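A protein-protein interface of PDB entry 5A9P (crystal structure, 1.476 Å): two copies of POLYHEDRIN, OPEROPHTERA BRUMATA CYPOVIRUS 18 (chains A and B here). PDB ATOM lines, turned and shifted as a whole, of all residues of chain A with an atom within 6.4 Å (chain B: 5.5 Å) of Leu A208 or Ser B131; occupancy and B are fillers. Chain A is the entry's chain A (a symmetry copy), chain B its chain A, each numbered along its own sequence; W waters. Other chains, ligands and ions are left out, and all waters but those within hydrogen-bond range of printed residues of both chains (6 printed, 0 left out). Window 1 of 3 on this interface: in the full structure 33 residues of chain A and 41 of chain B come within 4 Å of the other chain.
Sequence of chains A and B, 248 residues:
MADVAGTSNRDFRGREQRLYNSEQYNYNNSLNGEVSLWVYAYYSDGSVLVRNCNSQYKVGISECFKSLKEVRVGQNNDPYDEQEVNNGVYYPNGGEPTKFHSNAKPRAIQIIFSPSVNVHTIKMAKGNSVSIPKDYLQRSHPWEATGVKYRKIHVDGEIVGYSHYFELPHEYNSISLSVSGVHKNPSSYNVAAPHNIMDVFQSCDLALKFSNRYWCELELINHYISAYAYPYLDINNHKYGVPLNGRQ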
ATOM      1  N   GLU A  34      14.998  36.333  -2.416  1.00  0.00           N
ATOM      2  CA  GLU A  34      15.263  35.689  -3.690  1.00  0.00           C
ATOM      3  C   GLU A  34      15.071  36.649  -4.850  1.00  0.00           C
ATOM      4  O   GLU A  34      14.263  37.582  -4.770  1.00  0.00           O
ATOM      5  CB  GLU A  34      14.278  34.535  -3.896  1.00  0.00           C
ATOM      6  CG  GLU A  34      14.426  33.380  -2.926  1.00  0.00           C
ATOM      7  CD  GLU A  34      15.499  32.391  -3.335  1.00  0.00           C
ATOM      8  OE1 GLU A  34      16.265  32.682  -4.274  1.00  0.00           O
ATOM      9  OE2 GLU A  34      15.560  31.308  -2.716  1.00  0.00           O
ATOM     10  N   ASN A  52      14.308  26.878 -14.364  1.00  0.00           N
ATOM     11  CA  ASN A  52      14.154  27.861 -13.306  1.00  0.00           C
ATOM     12  C   ASN A  52      15.429  27.924 -12.486  1.00  0.00           C
ATOM     13  O   ASN A  52      16.095  26.904 -12.272  1.00  0.00           O
ATOM     14  CB  ASN A  52      12.944  27.483 -12.437  1.00  0.00           C
ATOM     15  CG  ASN A  52      12.875  28.245 -11.130  1.00  0.00           C
ATOM     16  OD1 ASN A  52      12.715  27.644 -10.067  1.00  0.00           O
ATOM     17  ND2 ASN A  52      12.962  29.565 -11.197  1.00  0.00           N
ATOM     18  N   CYS A  53      15.784  29.131 -12.061  1.00  0.00           N
ATOM     19  CA  CYS A  53      16.834  29.313 -11.070  1.00  0.00           C
ATOM     20  C   CYS A  53      16.389  30.355 -10.056  1.00  0.00           C
ATOM     21  O   CYS A  53      15.834  31.391 -10.426  1.00  0.00           O
ATOM     22  CB  CYS A  53      18.150  29.729 -11.718  1.00  0.00           C
ATOM     23  SG  CYS A  53      19.543  29.739 -10.551  1.00  0.00           S
ATOM     24  N   ASN A  54      16.633  30.054  -8.784  1.00  0.00           N
ATOM     25  CA  ASN A  54      16.270  30.919  -7.676  1.00  0.00           C
ATOM     26  C   ASN A  54      17.499  31.193  -6.842  1.00  0.00           C
ATOM     27  O   ASN A  54      18.118  30.262  -6.326  1.00  0.00           O
ATOM     28  CB  ASN A  54      15.227  30.234  -6.798  1.00  0.00           C
ATOM     29  CG  ASN A  54      14.016  29.790  -7.577  1.00  0.00           C
ATOM     30  OD1 ASN A  54      13.397  30.581  -8.279  1.00  0.00           O
ATOM     31  ND2 ASN A  54      13.681  28.514  -7.475  1.00  0.00           N
ATOM     32  N   SER A  55      17.861  32.463  -6.707  1.00  0.00           N
ATOM     33  CA  SER A  55      19.062  32.792  -5.959  1.00  0.00           C
ATOM     34  C   SER A  55      19.020  34.186  -5.364  1.00  0.00           C
ATOM     35  O   SER A  55      18.262  35.045  -5.794  1.00  0.00           O
ATOM     36  CB  SER A  55      20.297  32.656  -6.849  1.00  0.00           C
ATOM     37  OG  SER A  55      21.468  32.492  -6.068  1.00  0.00           O
ATOM     38  N   SER A 203      26.393  32.661  -3.140  1.00  0.00           N
ATOM     39  CA  SER A 203      25.069  32.621  -3.756  1.00  0.00           C
ATOM     40  C   SER A 203      25.115  31.907  -5.110  1.00  0.00           C
ATOM     41  O   SER A 203      24.117  31.318  -5.548  1.00  0.00           O
ATOM     42  CB  SER A 203      24.481  34.029  -3.902  1.00  0.00           C
ATOM     43  OG  SER A 203      24.983  34.697  -5.047  1.00  0.00           O
ATOM     44  N   ASP A 205      26.950  29.302  -5.627  1.00  0.00           N
ATOM     45  CA  ASP A 205      26.943  27.903  -5.213  1.00  0.00           C
ATOM     46  C   ASP A 205      25.536  27.489  -4.792  1.00  0.00           C
ATOM     47  O   ASP A 205      25.100  26.363  -5.023  1.00  0.00           O
ATOM     48  CB  ASP A 205      27.833  27.685  -3.979  1.00  0.00           C
ATOM     49  CG  ASP A 205      29.301  28.028  -4.203  1.00  0.00           C
ATOM     50  OD1 ASP A 205      29.795  27.913  -5.339  1.00  0.00           O
ATOM     51  OD2 ASP A 205      29.975  28.382  -3.201  1.00  0.00           O
ATOM     52  N   LEU A 206      24.852  28.408  -4.124  1.00  0.00           N
ATOM     53  CA  LEU A 206      23.624  28.095  -3.413  1.00  0.00           C
ATOM     54  C   LEU A 206      22.367  28.196  -4.274  1.00  0.00           C
ATOM     55  O   LEU A 206      21.306  27.695  -3.897  1.00  0.00           O
ATOM     56  CB  LEU A 206      23.498  29.013  -2.202  1.00  0.00           C
ATOM     57  CG  LEU A 206      24.492  28.745  -1.079  1.00  0.00           C
ATOM     58  CD1 LEU A 206      24.594  29.962  -0.174  1.00  0.00           C
ATOM     59  CD2 LEU A 206      24.084  27.494  -0.296  1.00  0.00           C
ATOM     60  N   ALA A 207      22.495  28.850  -5.424  1.00  0.00           N
ATOM     61  CA  ALA A 207      21.388  28.983  -6.356  1.00  0.00           C
ATOM     62  C   ALA A 207      20.763  27.620  -6.605  1.00  0.00           C
ATOM     63  O   ALA A 207      21.474  26.658  -6.912  1.00  0.00           O
ATOM     64  CB  ALA A 207      21.883  29.573  -7.658  1.00  0.00           C
ATOM     65  N   LEU A 208      19.444  27.542  -6.450  1.00  0.00           N
ATOM     66  CA  LEU A 208      18.711  26.309  -6.697  1.00  0.00           C
ATOM     67  C   LEU A 208      18.101  26.319  -8.090  1.00  0.00           C
ATOM     68  O   LEU A 208      17.506  27.315  -8.517  1.00  0.00           O
ATOM     69  CB  LEU A 208      17.617  26.104  -5.653  1.00  0.00           C
ATOM     70  CG  LEU A 208      18.068  25.784  -4.229  1.00  0.00           C
ATOM     71  CD1 LEU A 208      16.858  25.694  -3.316  1.00  0.00           C
ATOM     72  CD2 LEU A 208      18.875  24.490  -4.175  1.00  0.00           C
ATOM     73  N   LYS A 209      18.253  25.201  -8.785  1.00  0.00           N
ATOM     74  CA  LYS A 209      17.788  25.074 -10.152  1.00  0.00           C
ATOM     75  C   LYS A 209      16.708  24.011 -10.242  1.00  0.00           C
ATOM     76  O   LYS A 209      16.699  23.057  -9.465  1.00  0.00           O
ATOM     77  CB  LYS A 209      18.956  24.708 -11.060  1.00  0.00           C
ATOM     78  CG  LYS A 209      20.114  25.688 -10.975  1.00  0.00           C
ATOM     79  CD  LYS A 209      21.104  25.487 -12.113  1.00  0.00           C
ATOM     80  CE  LYS A 209      21.689  24.084 -12.153  1.00  0.00           C
ATOM     81  NZ  LYS A 209      22.564  23.788 -10.984  1.00  0.00           N
ATOM     82  N   PHE A 210      15.796  24.198 -11.190  1.00  0.00           N
ATOM     83  CA  PHE A 210      14.724  23.247 -11.446  1.00  0.00           C
ATOM     84  C   PHE A 210      14.469  23.181 -12.939  1.00  0.00           C
ATOM     85  O   PHE A 210      14.479  24.204 -13.623  1.00  0.00           O
ATOM     86  CB  PHE A 210      13.444  23.674 -10.733  1.00  0.00           C
ATOM     87  CG  PHE A 210      12.240  22.840 -11.090  1.00  0.00           C
ATOM     88  CD1 PHE A 210      11.964  21.667 -10.404  1.00  0.00           C
ATOM     89  CD2 PHE A 210      11.379  23.231 -12.101  1.00  0.00           C
ATOM     90  CE1 PHE A 210      10.856  20.908 -10.721  1.00  0.00           C
ATOM     91  CE2 PHE A 210      10.267  22.473 -12.419  1.00  0.00           C
ATOM     92  CZ  PHE A 210      10.011  21.308 -11.735  1.00  0.00           C
ATOM     93  N   SER A 211      14.240  21.969 -13.433  1.00  0.00           N
ATOM     94  CA  SER A 211      13.863  21.754 -14.820  1.00  0.00           C
ATOM     95  C   SER A 211      12.813  20.652 -14.920  1.00  0.00           C
ATOM     96  O   SER A 211      12.916  19.621 -14.248  1.00  0.00           O
ATOM     97  CB  SER A 211      15.091  21.382 -15.654  1.00  0.00           C
ATOM     98  OG  SER A 211      14.741  21.195 -17.016  1.00  0.00           O
ATOM     99  N   TYR A 230       3.896  31.430  -8.464  1.00  0.00           N
ATOM    100  CA  TYR A 230       4.787  32.026  -9.442  1.00  0.00           C
ATOM    101  C   TYR A 230       3.997  32.877 -10.413  1.00  0.00           C
ATOM    102  O   TYR A 230       2.829  32.589 -10.664  1.00  0.00           O
ATOM    103  CB  TYR A 230       5.452  30.935 -10.270  1.00  0.00           C
ATOM    104  CG  TYR A 230       6.446  30.056  -9.554  1.00  0.00           C
ATOM    105  CD1 TYR A 230       6.940  30.385  -8.299  1.00  0.00           C
ATOM    106  CD2 TYR A 230       6.907  28.897 -10.155  1.00  0.00           C
ATOM    107  CE1 TYR A 230       7.868  29.575  -7.665  1.00  0.00           C
ATOM    108  CE2 TYR A 230       7.821  28.086  -9.530  1.00  0.00           C
ATOM    109  CZ  TYR A 230       8.300  28.426  -8.287  1.00  0.00           C
ATOM    110  OH  TYR A 230       9.235  27.612  -7.692  1.00  0.00           O
ATOM    111  N   SER B  62      25.277  22.224  -6.005  1.00  0.00           N
ATOM    112  CA  SER B  62      23.845  22.497  -6.109  1.00  0.00           C
ATOM    113  C   SER B  62      23.148  21.393  -6.880  1.00  0.00           C
ATOM    114  O   SER B  62      23.502  21.094  -8.019  1.00  0.00           O
ATOM    115  CB  SER B  62      23.585  23.840  -6.787  1.00  0.00           C
ATOM    116  OG  SER B  62      22.199  24.142  -6.758  1.00  0.00           O
ATOM    117  N   GLU B  63      22.152  20.797  -6.240  1.00  0.00           N
ATOM    118  CA  GLU B  63      21.423  19.670  -6.792  1.00  0.00           C
ATOM    119  C   GLU B  63      19.932  19.946  -6.699  1.00  0.00           C
ATOM    120  O   GLU B  63      19.482  20.722  -5.860  1.00  0.00           O
ATOM    121  CB  GLU B  63      21.736  18.400  -6.002  1.00  0.00           C
ATOM    122  CG  GLU B  63      23.213  18.036  -5.956  1.00  0.00           C
ATOM    123  CD  GLU B  63      23.769  17.638  -7.312  1.00  0.00           C
ATOM    124  OE1 GLU B  63      22.989  17.168  -8.172  1.00  0.00           O
ATOM    125  OE2 GLU B  63      24.992  17.789  -7.517  1.00  0.00           O
ATOM    126  N   CYS B  64      19.174  19.298  -7.569  1.00  0.00           N
ATOM    127  CA  CYS B  64      17.722  19.395  -7.547  1.00  0.00           C
ATOM    128  C   CYS B  64      17.177  18.039  -7.128  1.00  0.00           C
ATOM    129  O   CYS B  64      17.941  17.093  -6.904  1.00  0.00           O
ATOM    130  CB  CYS B  64      17.199  19.805  -8.925  1.00  0.00           C
ATOM    131  SG  CYS B  64      17.665  18.701 -10.280  1.00  0.00           S
ATOM    132  N   PHE B  65      15.860  17.937  -7.012  1.00  0.00           N
ATOM    133  CA  PHE B  65      15.266  16.672  -6.614  1.00  0.00           C
ATOM    134  C   PHE B  65      15.685  15.552  -7.564  1.00  0.00           C
ATOM    135  O   PHE B  65      16.096  14.470  -7.129  1.00  0.00           O
ATOM    136  CB  PHE B  65      13.743  16.764  -6.570  1.00  0.00           C
ATOM    137  CG  PHE B  65      13.089  15.442  -6.346  1.00  0.00           C
ATOM    138  CD1 PHE B  65      13.067  14.880  -5.083  1.00  0.00           C
ATOM    139  CD2 PHE B  65      12.543  14.737  -7.401  1.00  0.00           C
ATOM    140  CE1 PHE B  65      12.496  13.646  -4.868  1.00  0.00           C
ATOM    141  CE2 PHE B  65      11.962  13.499  -7.192  1.00  0.00           C
ATOM    142  CZ  PHE B  65      11.941  12.957  -5.919  1.00  0.00           C
ATOM    143  N   ALA B 125      20.928  25.344   1.356  1.00  0.00           N
ATOM    144  CA  ALA B 125      19.532  25.457   0.956  1.00  0.00           C
ATOM    145  C   ALA B 125      18.965  24.058   0.733  1.00  0.00           C
ATOM    146  O   ALA B 125      19.139  23.458  -0.328  1.00  0.00           O
ATOM    147  CB  ALA B 125      19.392  26.302  -0.297  1.00  0.00           C
ATOM    148  N   GLY B 127      15.832  22.594   0.043  1.00  0.00           N
ATOM    149  CA  GLY B 127      14.551  23.085  -0.431  1.00  0.00           C
ATOM    150  C   GLY B 127      13.566  21.975  -0.716  1.00  0.00           C
ATOM    151  O   GLY B 127      13.849  20.802  -0.476  1.00  0.00           O
ATOM    152  N   ASN B 128      12.403  22.350  -1.235  1.00  0.00           N
ATOM    153  CA  ASN B 128      11.389  21.372  -1.599  1.00  0.00           C
ATOM    154  C   ASN B 128      11.667  20.768  -2.978  1.00  0.00           C
ATOM    155  O   ASN B 128      12.708  21.030  -3.587  1.00  0.00           O
ATOM    156  CB  ASN B 128       9.981  21.981  -1.513  1.00  0.00           C
ATOM    157  CG  ASN B 128       9.743  23.085  -2.528  1.00  0.00           C
ATOM    158  OD1 ASN B 128      10.522  23.278  -3.458  1.00  0.00           O
ATOM    159  ND2 ASN B 128       8.656  23.825  -2.343  1.00  0.00           N
ATOM    160  N   SER B 129      10.739  19.960  -3.472  1.00  0.00           N
ATOM    161  CA  SER B 129      11.008  19.172  -4.664  1.00  0.00           C
ATOM    162  C   SER B 129      11.063  20.020  -5.930  1.00  0.00           C
ATOM    163  O   SER B 129      11.532  19.552  -6.960  1.00  0.00           O
ATOM    164  CB  SER B 129       9.973  18.062  -4.818  1.00  0.00           C
ATOM    165  OG  SER B 129       8.689  18.602  -5.068  1.00  0.00           O
ATOM    166  N   VAL B 130      10.597  21.266  -5.850  1.00  0.00           N
ATOM    167  CA  VAL B 130      10.656  22.177  -7.001  1.00  0.00           C
ATOM    168  C   VAL B 130      11.672  23.299  -6.781  1.00  0.00           C
ATOM    169  O   VAL B 130      11.625  24.331  -7.449  1.00  0.00           O
ATOM    170  CB  VAL B 130       9.263  22.738  -7.380  1.00  0.00           C
ATOM    171  CG1 VAL B 130       8.339  21.600  -7.772  1.00  0.00           C
ATOM    172  CG2 VAL B 130       8.658  23.561  -6.247  1.00  0.00           C
ATOM    173  N   SER B 131      12.592  23.078  -5.846  1.00  0.00           N
ATOM    174  CA  SER B 131      13.770  23.932  -5.682  1.00  0.00           C
ATOM    175  C   SER B 131      13.473  25.317  -5.104  1.00  0.00           C
ATOM    176  O   SER B 131      14.067  26.315  -5.523  1.00  0.00           O
ATOM    177  CB  SER B 131      14.544  24.043  -7.008  1.00  0.00           C
ATOM    178  OG  SER B 131      14.964  22.755  -7.446  1.00  0.00           O
ATOM    179  N   ILE B 132      12.552  25.348  -4.137  1.00  0.00           N
ATOM    180  CA  ILE B 132      12.291  26.520  -3.305  1.00  0.00           C
ATOM    181  C   ILE B 132      12.817  26.239  -1.899  1.00  0.00           C
ATOM    182  O   ILE B 132      12.534  25.185  -1.343  1.00  0.00           O
ATOM    183  CB  ILE B 132      10.776  26.810  -3.207  1.00  0.00           C
ATOM    184  CG1 ILE B 132      10.178  27.029  -4.598  1.00  0.00           C
ATOM    185  CG2 ILE B 132      10.519  28.023  -2.307  1.00  0.00           C
ATOM    186  CD1 ILE B 132       8.651  27.136  -4.586  1.00  0.00           C
ATOM    187  N   PRO B 133      13.586  27.170  -1.310  1.00  0.00           N
ATOM    188  CA  PRO B 133      14.130  26.878   0.025  1.00  0.00           C
ATOM    189  C   PRO B 133      13.084  26.625   1.114  1.00  0.00           C
ATOM    190  O   PRO B 133      13.242  25.654   1.853  1.00  0.00           O
ATOM    191  CB  PRO B 133      14.952  28.131   0.349  1.00  0.00           C
ATOM    192  CG  PRO B 133      15.349  28.655  -0.976  1.00  0.00           C
ATOM    193  CD  PRO B 133      14.148  28.418  -1.857  1.00  0.00           C
ATOM    194  N   LEU B 137       8.798  31.161  -2.596  1.00  0.00           N
ATOM    195  CA  LEU B 137       9.938  32.041  -2.799  1.00  0.00           C
ATOM    196  C   LEU B 137       9.816  33.326  -1.988  1.00  0.00           C
ATOM    197  O   LEU B 137      10.808  33.845  -1.491  1.00  0.00           O
ATOM    198  CB  LEU B 137      10.072  32.382  -4.286  1.00  0.00           C
ATOM    199  CG  LEU B 137      10.542  31.248  -5.201  1.00  0.00           C
ATOM    200  CD1 LEU B 137      10.377  31.643  -6.650  1.00  0.00           C
ATOM    201  CD2 LEU B 137      11.991  30.880  -4.909  1.00  0.00           C
ATOM    202  N   SER B 176      15.419  19.348  -2.616  1.00  0.00           N
ATOM    203  CA  SER B 176      16.482  19.855  -3.466  1.00  0.00           C
ATOM    204  C   SER B 176      17.556  20.296  -2.492  1.00  0.00           C
ATOM    205  O   SER B 176      17.279  20.443  -1.298  1.00  0.00           O
ATOM    206  CB  SER B 176      15.995  21.028  -4.312  1.00  0.00           C
ATOM    207  OG  SER B 176      15.329  21.987  -3.509  1.00  0.00           O
ATOM    208  N   LEU B 177      18.778  20.505  -2.964  1.00  0.00           N
ATOM    209  CA  LEU B 177      19.875  20.742  -2.031  1.00  0.00           C
ATOM    210  C   LEU B 177      21.043  21.487  -2.636  1.00  0.00           C
ATOM    211  O   LEU B 177      21.647  21.025  -3.601  1.00  0.00           O
ATOM    212  CB  LEU B 177      20.394  19.406  -1.482  1.00  0.00           C
ATOM    213  CG  LEU B 177      21.479  19.509  -0.401  1.00  0.00           C
ATOM    214  CD1 LEU B 177      20.971  20.237   0.828  1.00  0.00           C
ATOM    215  CD2 LEU B 177      22.001  18.129  -0.020  1.00  0.00           C
ATOM    216  N   SER B 178      21.384  22.624  -2.039  1.00  0.00           N
ATOM    217  CA  SER B 178      22.665  23.247  -2.328  1.00  0.00           C
ATOM    218  C   SER B 178      23.419  23.495  -1.028  1.00  0.00           C
ATOM    219  O   SER B 178      22.817  23.699   0.028  1.00  0.00           O
ATOM    220  CB  SER B 178      22.482  24.542  -3.111  1.00  0.00           C
ATOM    221  OG  SER B 178      21.799  25.488  -2.324  1.00  0.00           O
HETATM  222  O   HOH W   1      19.899  23.029  -7.743  1.00  0.00           O
HETATM  223  O   HOH W   2      23.225  26.413  -9.145  1.00  0.00           O
HETATM  224  O   HOH W   3      10.707  25.928  -9.431  1.00  0.00           O
HETATM  225  O   HOH W   4      15.044  19.480 -12.214  1.00  0.00           O
HETATM  226  O   HOH W   5      12.666  35.743  -0.730  1.00  0.00           O
HETATM  227  O   HOH W   6      27.143  24.808  -6.615  1.00  0.00           O
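Printed residues of chain B within 4 Å of Leu A208: Ala B125 (3.99 Å), Ser B131 (3.6 Å) and Ser B178 (3.6 Å).
Printed residues of chain A within 4 Å of Ser B131: Asn A54 (3.0 Å), Leu A208 (3.6 Å), Lys A209 (2.7 Å) and Phe A210 (3.7 Å).
Printed residues of chain B within 4 Å of Lys A209: Cys B64 and Ser B131.
Of the printed residues of chain B, Asn A54 touches Ser B131 and Leu B137.
Ser B176 touches none of the printed residues of chain A.
Asn B128 touches none of the printed residues of chain A.
The nearest printed residue of chain B that does not touch Glu A34 is Ile B132 (5.8 Å).
The backbone carbonyl oxygen (O) of Ala A207 lies within hydrogen-bond range of the side-chain hydroxyl (OG) of Ser B62 (2.6 Å).
O of Ser B131 is in hydrogen-bond range of ND2 of Asn A54, at 3.0 Å.
O of Lys A209 is in hydrogen-bond range of OG of Ser B131 (2.7 Å).
OG of Ser B178 lies within hydrogen-bond range of O of Leu A206 (2.8 Å).
Water W3 lies within hydrogen-bond range of the backbone carbonyl oxygen of Val B130, the side-chain amide oxygen of Asn A52 and the side-chain hydroxyl of Tyr A230.
Water W1 lies within hydrogen-bond range of OG of Ser B62 (2.7 Å), N of Lys A209 (2.9 Å) and O of Glu B63 (3.0 Å).
Water W5 bridges O of Leu B137 (2.8 Å) and N of Glu A34 (2.9 Å).
Water W2 lies within hydrogen-bond range of O of Ala A207 (2.8 Å), NZ of Lys A209 (3.3 Å) and OG of Ser B62 (3.5 Å).
Water W4 bridges the backbone NH of Ser A211 (2.9 Å) and the side-chain sulfur of Cys B64 (3.3 Å).
Water W6 bridges the backbone carbonyl oxygen of Asp A205 (3.0 Å) and the backbone NH of Ser B62 (3.2 Å).
No position is printed for both chains.
Of the 17 pairs that touch across the chains among the printed residues, none has its exchanged pair printed and touching as well.
Of the 16 printed residues of chain B, 9 touch a printed residue of chain A.
Hydrophobic or aromatic side chains of chain B that line the printed part of chain A: Ala B125, Val B130, Ile B132, Pro B133 and Leu B137.
Among the printed residues, no Asp or Glu carboxylate lies within 4 Å of a Lys or Arg side-chain nitrogen of the other chain.
Among the printed residues, merely in contact across the chains: Glu A34 with Pro B133 (3.2 Å), Glu A34 with Leu B137 (3.9 Å), Asn A54 with Leu B137 (3.5 Å), Asp A205 with Ser B62 (3.4 Å), Asp A205 with Ser B178 (3.7 Å), Leu A208 with Ala B125 (3.99 Å), Leu A208 with Ser B131 (3.6 Å), Leu A208 with Ser B178 (3.6 Å), Lys A209 with Cys B64 (3.3 Å), Phe A210 with Val B130 (3.7 Å), Phe A210 with Ser B131 (3.7 Å), Tyr A230 with Ile B132 (3.2 Å) and Tyr A230 with Leu B137 (3.4 Å).
The side-chain amide oxygen (OD1) of Asn B128 lies close to the backbone NH (N) of Val B130 (3.1 Å).
The side-chain amide oxygen (OD1) of Asn B128 is in hydrogen-bond range of the backbone NH (N) of Ile B132 (3.0 Å).
The side-chain carboxylate (OE1) of Glu A34 sits at hydrogen-bond distance from the backbone NH (N) of Ser A55.
The side-chain amide oxygen of Asn A52 sits at hydrogen-bond distance from the side-chain amide nitrogen of Asn A54 (2.9 Å).
O of Phe A210 lies within hydrogen-bond range of N of Asn A52 (2.8 Å).
The side-chain sulfur of Cys A53 lies close to the backbone carbonyl oxygen of Leu A208.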
